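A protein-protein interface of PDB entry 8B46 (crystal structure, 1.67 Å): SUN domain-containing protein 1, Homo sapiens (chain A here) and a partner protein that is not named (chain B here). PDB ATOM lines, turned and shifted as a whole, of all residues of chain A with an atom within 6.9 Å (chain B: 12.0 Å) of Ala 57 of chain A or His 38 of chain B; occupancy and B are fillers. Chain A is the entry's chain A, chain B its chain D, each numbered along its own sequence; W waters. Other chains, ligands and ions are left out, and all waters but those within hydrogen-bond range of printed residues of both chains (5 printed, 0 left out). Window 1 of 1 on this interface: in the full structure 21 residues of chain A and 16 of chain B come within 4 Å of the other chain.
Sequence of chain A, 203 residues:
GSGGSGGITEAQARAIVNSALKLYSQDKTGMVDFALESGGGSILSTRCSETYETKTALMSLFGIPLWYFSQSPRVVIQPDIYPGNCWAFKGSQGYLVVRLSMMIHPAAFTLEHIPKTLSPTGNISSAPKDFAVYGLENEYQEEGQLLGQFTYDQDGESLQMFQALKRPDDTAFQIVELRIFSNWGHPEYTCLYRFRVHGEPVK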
ATOM      1  N   THR A  54      12.626 -28.249  -6.000  1.00  0.00           N
ATOM      2  CA  THR A  54      13.390 -29.311  -6.630  1.00  0.00           C
ATOM      3  C   THR A  54      14.842 -29.071  -6.250  1.00  0.00           C
ATOM      4  O   THR A  54      15.284 -27.913  -6.207  1.00  0.00           O
ATOM      5  CB  THR A  54      13.154 -29.248  -8.142  1.00  0.00           C
ATOM      6  OG1 THR A  54      14.090 -30.079  -8.822  1.00  0.00           O
ATOM      7  CG2 THR A  54      13.320 -27.774  -8.654  1.00  0.00           C
ATOM      8  N   LYS A  55      15.551 -30.118  -5.856  1.00  0.00           N
ATOM      9  CA  LYS A  55      16.980 -30.000  -5.586  1.00  0.00           C
ATOM     10  C   LYS A  55      17.777 -30.620  -6.716  1.00  0.00           C
ATOM     11  O   LYS A  55      18.806 -31.253  -6.482  1.00  0.00           O
ATOM     12  CB  LYS A  55      17.424 -30.654  -4.278  1.00  0.00           C
ATOM     13  CG  LYS A  55      17.108 -29.921  -2.976  1.00  0.00           C
ATOM     14  CD  LYS A  55      17.931 -30.594  -1.863  1.00  0.00           C
ATOM     15  CE  LYS A  55      17.844 -29.877  -0.522  1.00  0.00           C
ATOM     16  NZ  LYS A  55      18.878 -30.439   0.458  1.00  0.00           N
ATOM     17  N   THR A  56      17.345 -30.427  -7.958  1.00  0.00           N
ATOM     18  CA  THR A  56      18.039 -31.109  -9.040  1.00  0.00           C
ATOM     19  C   THR A  56      18.880 -30.200  -9.923  1.00  0.00           C
ATOM     20  O   THR A  56      19.668 -30.719 -10.718  1.00  0.00           O
ATOM     21  CB  THR A  56      17.039 -31.867  -9.927  1.00  0.00           C
ATOM     22  OG1 THR A  56      16.117 -30.936 -10.524  1.00  0.00           O
ATOM     23  CG2 THR A  56      16.282 -32.914  -9.090  1.00  0.00           C
ATOM     24  N   ALA A  57      18.738 -28.877  -9.834  1.00  0.00           N
ATOM     25  CA  ALA A  57      19.607 -27.971 -10.583  1.00  0.00           C
ATOM     26  C   ALA A  57      20.637 -27.392  -9.605  1.00  0.00           C
ATOM     27  O   ALA A  57      20.415 -26.360  -8.974  1.00  0.00           O
ATOM     28  CB  ALA A  57      18.782 -26.899 -11.255  1.00  0.00           C
ATOM     29  N   LEU A  58      21.767 -28.062  -9.466  1.00  0.00           N
ATOM     30  CA  LEU A  58      22.799 -27.644  -8.518  1.00  0.00           C
ATOM     31  C   LEU A  58      23.762 -26.606  -9.102  1.00  0.00           C
ATOM     32  O   LEU A  58      24.466 -26.867 -10.099  1.00  0.00           O
ATOM     33  CB  LEU A  58      23.586 -28.865  -8.056  1.00  0.00           C
ATOM     34  CG  LEU A  58      24.741 -28.583  -7.076  1.00  0.00           C
ATOM     35  CD1 LEU A  58      24.266 -27.968  -5.752  1.00  0.00           C
ATOM     36  CD2 LEU A  58      25.539 -29.837  -6.839  1.00  0.00           C
ATOM     37  N   MET A  59      23.850 -25.447  -8.442  1.00  0.00           N
ATOM     38  CA  MET A  59      24.853 -24.444  -8.739  1.00  0.00           C
ATOM     39  C   MET A  59      26.021 -24.736  -7.829  1.00  0.00           C
ATOM     40  O   MET A  59      25.846 -24.857  -6.597  1.00  0.00           O
ATOM     41  CB  MET A  59      24.337 -23.043  -8.431  1.00  0.00           C
ATOM     42  CG  MET A  59      23.026 -22.669  -9.116  1.00  0.00           C
ATOM     43  SD  MET A  59      22.964 -23.034 -10.917  1.00  0.00           S
ATOM     44  CE  MET A  59      24.203 -21.922 -11.510  1.00  0.00           C
ATOM     45  N   TRP A  67      24.037 -23.690  -4.272  1.00  0.00           N
ATOM     46  CA  TRP A  67      22.613 -23.529  -3.997  1.00  0.00           C
ATOM     47  C   TRP A  67      21.867 -24.249  -5.093  1.00  0.00           C
ATOM     48  O   TRP A  67      22.446 -24.562  -6.137  1.00  0.00           O
ATOM     49  CB  TRP A  67      22.184 -22.040  -3.901  1.00  0.00           C
ATOM     50  CG  TRP A  67      21.726 -21.354  -5.205  1.00  0.00           C
ATOM     51  CD1 TRP A  67      20.425 -21.314  -5.710  1.00  0.00           C
ATOM     52  CD2 TRP A  67      22.535 -20.624  -6.146  1.00  0.00           C
ATOM     53  NE1 TRP A  67      20.399 -20.585  -6.892  1.00  0.00           N
ATOM     54  CE2 TRP A  67      21.670 -20.155  -7.180  1.00  0.00           C
ATOM     55  CE3 TRP A  67      23.897 -20.288  -6.200  1.00  0.00           C
ATOM     56  CZ2 TRP A  67      22.131 -19.393  -8.260  1.00  0.00           C
ATOM     57  CZ3 TRP A  67      24.359 -19.515  -7.295  1.00  0.00           C
ATOM     58  CH2 TRP A  67      23.472 -19.094  -8.309  1.00  0.00           C
ATOM     59  N   TYR A  68      20.587 -24.531  -4.842  1.00  0.00           N
ATOM     60  CA  TYR A  68      19.715 -25.215  -5.798  1.00  0.00           C
ATOM     61  C   TYR A  68      18.865 -24.200  -6.562  1.00  0.00           C
ATOM     62  O   TYR A  68      18.143 -23.407  -5.954  1.00  0.00           O
ATOM     63  CB  TYR A  68      18.856 -26.256  -5.098  1.00  0.00           C
ATOM     64  CG  TYR A  68      19.730 -27.386  -4.596  1.00  0.00           C
ATOM     65  CD1 TYR A  68      20.198 -28.376  -5.461  1.00  0.00           C
ATOM     66  CD2 TYR A  68      20.124 -27.438  -3.263  1.00  0.00           C
ATOM     67  CE1 TYR A  68      21.001 -29.421  -4.996  1.00  0.00           C
ATOM     68  CE2 TYR A  68      20.918 -28.468  -2.784  1.00  0.00           C
ATOM     69  CZ  TYR A  68      21.375 -29.442  -3.656  1.00  0.00           C
ATOM     70  OH  TYR A  68      22.199 -30.433  -3.166  1.00  0.00           O
ATOM     71  N   PHE A  69      19.037 -24.153  -7.871  1.00  0.00           N
ATOM     72  CA  PHE A  69      18.346 -23.157  -8.683  1.00  0.00           C
ATOM     73  C   PHE A  69      16.905 -23.569  -8.991  1.00  0.00           C
ATOM     74  O   PHE A  69      16.621 -24.732  -9.317  1.00  0.00           O
ATOM     75  CB  PHE A  69      19.121 -22.943  -9.985  1.00  0.00           C
ATOM     76  CG  PHE A  69      18.454 -22.005 -10.927  1.00  0.00           C
ATOM     77  CD1 PHE A  69      18.494 -20.629 -10.709  1.00  0.00           C
ATOM     78  CD2 PHE A  69      17.740 -22.488 -11.997  1.00  0.00           C
ATOM     79  CE1 PHE A  69      17.870 -19.768 -11.557  1.00  0.00           C
ATOM     80  CE2 PHE A  69      17.087 -21.616 -12.844  1.00  0.00           C
ATOM     81  CZ  PHE A  69      17.143 -20.244 -12.610  1.00  0.00           C
ATOM     82  N   SER A  70      15.983 -22.622  -8.831  1.00  0.00           N
ATOM     83  CA  SER A  70      14.595 -22.772  -9.267  1.00  0.00           C
ATOM     84  C   SER A  70      14.127 -21.402  -9.774  1.00  0.00           C
ATOM     85  O   SER A  70      14.577 -20.365  -9.286  1.00  0.00           O
ATOM     86  CB  SER A  70      13.706 -23.327  -8.152  1.00  0.00           C
ATOM     87  OG  SER A  70      13.497 -22.325  -7.181  1.00  0.00           O
ATOM     88  N   TRP B  23      18.123 -11.201  -3.384  1.00  0.00           N
ATOM     89  CA  TRP B  23      18.619 -12.496  -3.837  1.00  0.00           C
ATOM     90  C   TRP B  23      18.822 -12.521  -5.349  1.00  0.00           C
ATOM     91  O   TRP B  23      19.822 -13.060  -5.838  1.00  0.00           O
ATOM     92  CB  TRP B  23      17.707 -13.650  -3.419  1.00  0.00           C
ATOM     93  CG  TRP B  23      18.112 -14.833  -4.217  1.00  0.00           C
ATOM     94  CD1 TRP B  23      17.433 -15.390  -5.264  1.00  0.00           C
ATOM     95  CD2 TRP B  23      19.369 -15.531  -4.135  1.00  0.00           C
ATOM     96  NE1 TRP B  23      18.169 -16.419  -5.808  1.00  0.00           N
ATOM     97  CE2 TRP B  23      19.359 -16.527  -5.137  1.00  0.00           C
ATOM     98  CE3 TRP B  23      20.489 -15.426  -3.295  1.00  0.00           C
ATOM     99  CZ2 TRP B  23      20.420 -17.410  -5.323  1.00  0.00           C
ATOM    100  CZ3 TRP B  23      21.547 -16.307  -3.487  1.00  0.00           C
ATOM    101  CH2 TRP B  23      21.502 -17.284  -4.493  1.00  0.00           C
ATOM    102  N   GLU B  27      22.112 -13.314  -7.369  1.00  0.00           N
ATOM    103  CA  GLU B  27      22.100 -14.387  -8.359  1.00  0.00           C
ATOM    104  C   GLU B  27      22.664 -13.901  -9.685  1.00  0.00           C
ATOM    105  O   GLU B  27      23.411 -14.629 -10.353  1.00  0.00           O
ATOM    106  CB  GLU B  27      20.673 -14.904  -8.526  1.00  0.00           C
ATOM    107  CG  GLU B  27      20.494 -16.208  -9.303  1.00  0.00           C
ATOM    108  CD  GLU B  27      19.052 -16.740  -9.194  1.00  0.00           C
ATOM    109  OE1 GLU B  27      18.108 -16.073  -9.686  1.00  0.00           O
ATOM    110  OE2 GLU B  27      18.855 -17.816  -8.584  1.00  0.00           O
ATOM    111  N   LEU B  30      26.305 -13.917  -9.324  1.00  0.00           N
ATOM    112  CA  LEU B  30      26.881 -15.253  -9.246  1.00  0.00           C
ATOM    113  C   LEU B  30      26.829 -15.999 -10.583  1.00  0.00           C
ATOM    114  O   LEU B  30      27.798 -16.677 -10.943  1.00  0.00           O
ATOM    115  CB  LEU B  30      26.175 -16.047  -8.157  1.00  0.00           C
ATOM    116  CG  LEU B  30      26.508 -15.479  -6.788  1.00  0.00           C
ATOM    117  CD1 LEU B  30      25.601 -16.098  -5.731  1.00  0.00           C
ATOM    118  CD2 LEU B  30      27.973 -15.753  -6.509  1.00  0.00           C
ATOM    119  N   TRP B  31      25.726 -15.861 -11.344  1.00  0.00           N
ATOM    120  CA  TRP B  31      25.351 -16.703 -12.481  1.00  0.00           C
ATOM    121  C   TRP B  31      26.528 -17.080 -13.382  1.00  0.00           C
ATOM    122  O   TRP B  31      26.812 -18.277 -13.508  1.00  0.00           O
ATOM    123  CB  TRP B  31      24.268 -16.032 -13.326  1.00  0.00           C
ATOM    124  CG  TRP B  31      23.549 -16.990 -14.286  1.00  0.00           C
ATOM    125  CD1 TRP B  31      23.516 -16.925 -15.679  1.00  0.00           C
ATOM    126  CD2 TRP B  31      22.739 -18.127 -13.923  1.00  0.00           C
ATOM    127  NE1 TRP B  31      22.739 -17.950 -16.179  1.00  0.00           N
ATOM    128  CE2 TRP B  31      22.258 -18.704 -15.132  1.00  0.00           C
ATOM    129  CE3 TRP B  31      22.365 -18.704 -12.696  1.00  0.00           C
ATOM    130  CZ2 TRP B  31      21.413 -19.824 -15.141  1.00  0.00           C
ATOM    131  CZ3 TRP B  31      21.549 -19.825 -12.707  1.00  0.00           C
ATOM    132  CH2 TRP B  31      21.076 -20.368 -13.923  1.00  0.00           C
ATOM    133  N   THR B  34      29.335 -19.569 -11.675  1.00  0.00           N
ATOM    134  CA  THR B  34      28.992 -20.854 -11.138  1.00  0.00           C
ATOM    135  C   THR B  34      28.867 -21.850 -12.280  1.00  0.00           C
ATOM    136  O   THR B  34      28.719 -21.472 -13.439  1.00  0.00           O
ATOM    137  CB  THR B  34      27.675 -20.755 -10.359  1.00  0.00           C
ATOM    138  OG1 THR B  34      26.658 -20.319 -11.257  1.00  0.00           O
ATOM    139  CG2 THR B  34      27.806 -19.726  -9.201  1.00  0.00           C
ATOM    140  N   ARG B  35      28.898 -23.138 -11.927  1.00  0.00           N
ATOM    141  CA  ARG B  35      28.609 -24.226 -12.849  1.00  0.00           C
ATOM    142  C   ARG B  35      27.243 -24.743 -12.475  1.00  0.00           C
ATOM    143  O   ARG B  35      26.839 -24.624 -11.324  1.00  0.00           O
ATOM    144  CB  ARG B  35      29.659 -25.325 -12.745  1.00  0.00           C
ATOM    145  CG  ARG B  35      31.036 -24.796 -13.031  1.00  0.00           C
ATOM    146  CD  ARG B  35      31.088 -24.179 -14.485  1.00  0.00           C
ATOM    147  NE  ARG B  35      32.333 -23.473 -14.800  1.00  0.00           N
ATOM    148  CZ  ARG B  35      32.436 -22.151 -14.926  1.00  0.00           C
ATOM    149  NH1 ARG B  35      31.364 -21.361 -14.881  1.00  0.00           N
ATOM    150  NH2 ARG B  35      33.641 -21.605 -15.114  1.00  0.00           N
ATOM    151  N   LEU B  36      26.523 -25.298 -13.444  1.00  0.00           N
ATOM    152  CA  LEU B  36      25.166 -25.794 -13.218  1.00  0.00           C
ATOM    153  C   LEU B  36      25.116 -27.251 -13.664  1.00  0.00           C
ATOM    154  O   LEU B  36      25.414 -27.555 -14.825  1.00  0.00           O
ATOM    155  CB  LEU B  36      24.145 -24.944 -13.987  1.00  0.00           C
ATOM    156  CG  LEU B  36      22.710 -25.472 -14.097  1.00  0.00           C
ATOM    157  CD1 LEU B  36      22.173 -25.960 -12.758  1.00  0.00           C
ATOM    158  CD2 LEU B  36      21.842 -24.335 -14.646  1.00  0.00           C
ATOM    159  N   ARG B  37      24.791 -28.146 -12.731  1.00  0.00           N
ATOM    160  CA  ARG B  37      24.605 -29.562 -13.029  1.00  0.00           C
ATOM    161  C   ARG B  37      23.144 -29.922 -12.810  1.00  0.00           C
ATOM    162  O   ARG B  37      22.610 -29.742 -11.705  1.00  0.00           O
ATOM    163  CB  ARG B  37      25.482 -30.451 -12.148  1.00  0.00           C
ATOM    164  CG  ARG B  37      25.025 -31.912 -12.283  1.00  0.00           C
ATOM    165  CD  ARG B  37      25.731 -32.861 -11.328  1.00  0.00           C
ATOM    166  NE  ARG B  37      26.922 -33.366 -11.983  1.00  0.00           N
ATOM    167  CZ  ARG B  37      26.925 -34.391 -12.824  1.00  0.00           C
ATOM    168  NH1 ARG B  37      25.820 -35.091 -13.077  1.00  0.00           N
ATOM    169  NH2 ARG B  37      28.062 -34.721 -13.424  1.00  0.00           N
ATOM    170  N   HIS B  38      22.494 -30.449 -13.840  1.00  0.00           N
ATOM    171  CA  HIS B  38      21.184 -31.046 -13.631  1.00  0.00           C
ATOM    172  C   HIS B  38      21.369 -32.494 -13.221  1.00  0.00           C
ATOM    173  O   HIS B  38      22.062 -33.250 -13.908  1.00  0.00           O
ATOM    174  CB  HIS B  38      20.334 -30.953 -14.886  1.00  0.00           C
ATOM    175  CG  HIS B  38      20.108 -29.549 -15.332  1.00  0.00           C
ATOM    176  ND1 HIS B  38      19.165 -28.723 -14.759  1.00  0.00           N
ATOM    177  CD2 HIS B  38      20.678 -28.838 -16.324  1.00  0.00           C
ATOM    178  CE1 HIS B  38      19.187 -27.548 -15.373  1.00  0.00           C
ATOM    179  NE2 HIS B  38      20.071 -27.605 -16.343  1.00  0.00           N
ATOM    180  N   ASN B  39      20.795 -32.865 -12.079  1.00  0.00           N
ATOM    181  CA  ASN B  39      20.786 -34.245 -11.628  1.00  0.00           C
ATOM    182  C   ASN B  39      19.495 -34.932 -11.972  1.00  0.00           C
ATOM    183  O   ASN B  39      19.304 -36.078 -11.594  1.00  0.00           O
ATOM    184  CB  ASN B  39      21.048 -34.321 -10.119  1.00  0.00           C
ATOM    185  CG  ASN B  39      22.529 -34.137  -9.808  1.00  0.00           C
ATOM    186  OD1 ASN B  39      23.388 -34.821 -10.412  1.00  0.00           O
ATOM    187  ND2 ASN B  39      22.851 -33.179  -8.923  1.00  0.00           N
ATOM    188  N   GLY B  40      18.613 -34.252 -12.671  1.00  0.00           N
ATOM    189  CA  GLY B  40      17.354 -34.785 -13.125  1.00  0.00           C
ATOM    190  C   GLY B  40      16.790 -33.638 -13.930  1.00  0.00           C
ATOM    191  O   GLY B  40      17.318 -32.518 -13.882  1.00  0.00           O
ATOM    192  N   PRO B  41      15.759 -33.885 -14.725  1.00  0.00           N
ATOM    193  CA  PRO B  41      15.236 -32.827 -15.621  1.00  0.00           C
ATOM    194  C   PRO B  41      14.623 -31.678 -14.830  1.00  0.00           C
ATOM    195  O   PRO B  41      13.839 -31.897 -13.902  1.00  0.00           O
ATOM    196  CB  PRO B  41      14.167 -33.568 -16.442  1.00  0.00           C
ATOM    197  CG  PRO B  41      13.790 -34.767 -15.561  1.00  0.00           C
ATOM    198  CD  PRO B  41      15.061 -35.173 -14.884  1.00  0.00           C
ATOM    199  N   PRO B  42      14.943 -30.434 -15.172  1.00  0.00           N
ATOM    200  CA  PRO B  42      14.273 -29.273 -14.539  1.00  0.00           C
ATOM    201  C   PRO B  42      12.838 -29.179 -15.032  1.00  0.00           C
ATOM    202  O   PRO B  42      12.495 -29.822 -16.030  1.00  0.00           O
ATOM    203  CB  PRO B  42      15.112 -28.084 -15.039  1.00  0.00           C
ATOM    204  CG  PRO B  42      15.538 -28.523 -16.439  1.00  0.00           C
ATOM    205  CD  PRO B  42      15.799 -30.043 -16.306  1.00  0.00           C
ATOM    206  N   PRO B  43      11.964 -28.404 -14.391  1.00  0.00           N
ATOM    207  CA  PRO B  43      10.602 -28.269 -14.943  1.00  0.00           C
ATOM    208  C   PRO B  43      10.656 -27.593 -16.309  1.00  0.00           C
ATOM    209  O   PRO B  43      11.354 -26.600 -16.494  1.00  0.00           O
ATOM    210  CB  PRO B  43       9.878 -27.404 -13.913  1.00  0.00           C
ATOM    211  CG  PRO B  43      10.690 -27.628 -12.586  1.00  0.00           C
ATOM    212  CD  PRO B  43      12.125 -27.703 -13.092  1.00  0.00           C
ATOM    213  N   VAL B  44       9.968 -28.169 -17.296  1.00  0.00           N
ATOM    214  CA  VAL B  44       9.862 -27.504 -18.615  1.00  0.00           C
ATOM    215  C   VAL B  44       8.412 -27.604 -19.050  1.00  0.00           C
ATOM    216  O   VAL B  44       7.901 -26.886 -19.943  1.00  0.00           O
ATOM    217  CB  VAL B  44      10.814 -28.118 -19.731  1.00  0.00           C
ATOM    218  CG1 VAL B  44      12.277 -28.066 -19.359  1.00  0.00           C
ATOM    219  CG2 VAL B  44      10.387 -29.537 -20.106  1.00  0.00           C
ATOM    220  OXT VAL B  44       7.699 -28.463 -18.511  1.00  0.00           O
HETATM  221  O   HOH W   1      17.126 -29.886 -12.744  1.00  0.00           O
HETATM  222  O   HOH W   2      27.268 -27.767 -10.232  1.00  0.00           O
HETATM  223  O   HOH W   3      15.575 -17.566  -9.264  1.00  0.00           O
HETATM  224  O   HOH W   4      21.346 -32.590  -6.990  1.00  0.00           O
HETATM  225  O   HOH W   5      14.375 -33.189 -11.407  1.00  0.00           O
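The backbone carbonyl oxygen of Arg 37 of chain B sits close to the backbone carbonyl oxygen of Thr 56 of chain A, at 3.3 Å. The backbone carbonyl oxygen of Arg 37 of chain B is in hydrogen-bond range of the backbone NH of Leu 58 of chain A, at 2.9 Å. The backbone NH (N) of Asn 39 of chain B sits at hydrogen-bond distance from the backbone carbonyl oxygen (O) of Thr 56 of chain A. The backbone carbonyl oxygen of Leu 58 of chain A sits close to the backbone carbonyl oxygen of Arg 35 of chain B.
The backbone NH (N) of Phe 69 of chain A is in hydrogen-bond range of the backbone carbonyl oxygen (O) of Ala 57 of chain A (2.8 Å). OG1 of Thr 54 of chain A sits at hydrogen-bond distance from OG1 of Thr 56 of chain A. The indole nitrogen (NE1) of Trp 23 of chain B is in hydrogen-bond range of the side-chain carboxylate (OE2) of Glu 27 of chain B, at 3.2 Å. The backbone carbonyl oxygen of Trp 31 of chain B lies within hydrogen-bond range of the side-chain hydroxyl of Thr 34 of chain B, at 3.0 Å. The backbone NH (N) of Met 59 of chain A lies within hydrogen-bond range of the backbone carbonyl oxygen (O) of Trp 67 of chain A (2.8 Å).
OG1 of Thr 56 of chain A touches O of Gly 40 of chain B, 3.9 Å away. CD1 of Leu 36 of chain B touches C of Ala 57 of chain A (3.8 Å). Leu 36 of chain B touches Leu 58 of chain A. Thr 34 of chain B touches Met 59 of chain A. CD1 of Leu 36 of chain B touches SD of Met 59 of chain A, 3.5 Å away. NE1 of Trp 67 of chain A touches CZ2 of Trp 23 of chain B, 3.5 Å away. Glu 27 of chain B touches Trp 67 of chain A. CZ3 of Trp 67 of chain A touches CD1 of Leu 30 of chain B, 3.96 Å away. CG2 of Thr 34 of chain B touches CZ3 of Trp 67 of chain A (3.9 Å). Trp 31 of chain B touches Phe 69 of chain A (CZ3 to CD1, 3.7 Å).
No residue of chain B comes within 4 Å of Thr 54 of chain A. Met 59 of chain A touches just these residues of chain B: Trp 31 (3.6 Å), Thr 34 (2.9 Å), Arg 35 (3.3 Å) and Leu 36 (3.5 Å). Of the printed residues of chain B, Trp 67 of chain A touches Trp 23 (3.5 Å), Glu 27 (3.6 Å), Leu 30 (3.96 Å) and Thr 34 (3.9 Å). Of chain A, only Thr 56 and Ala 57 come within 4 Å of His 38 of chain B. Of the printed residues of chain A, Gly 40 of chain B touches Thr 56. Pro 41 of chain B touches none of the printed residues of chain A. Val 44 of chain B touches none of the printed residues of chain A. The nearest printed residue of chain A that does not touch Gly 40 of chain B is Ala 57 of chain A (5.6 Å).
Of the 10 printed residues of chain A, 6 touch a printed residue of chain B. Printed residues of chain B that touch a printed residue of chain A: Trp 23, Glu 27, Leu 30, Trp 31, Thr 34, Arg 35, Leu 36, Arg 37, His 38, Asn 39 and Gly 40. Hydrophobic or aromatic side chains of chain B that line the printed part of chain A: Trp 23, Leu 30, Trp 31, Leu 36 and His 38. Among the printed residues, no Asp or Glu carboxylate lies within 4 Å of a Lys or Arg side-chain nitrogen of the other chain.
Water W4 lies within hydrogen-bond range of ND2 of Asn 39 of chain B (2.5 Å) and O of Lys 55 of chain A (2.9 Å). Water W1 lies within hydrogen-bond range of the side-chain hydroxyl of Thr 56 of chain A, the backbone carbonyl oxygen of Gly 40 of chain B, a ring nitrogen (ND1) of His 38 of chain B and the backbone NH of Ala 57 of chain A. Water W5 bridges O of Pro 41 of chain B (2.9 Å) and OG1 of Thr 56 of chain A (3.0 Å). Water W2 bridges O of Leu 58 of chain A (2.9 Å) and O of Arg 35 of chain B (3.4 Å). Water W3 bridges OE1 of Glu 27 of chain B (3.0 Å) and O of Ser 70 of chain A (3.0 Å).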
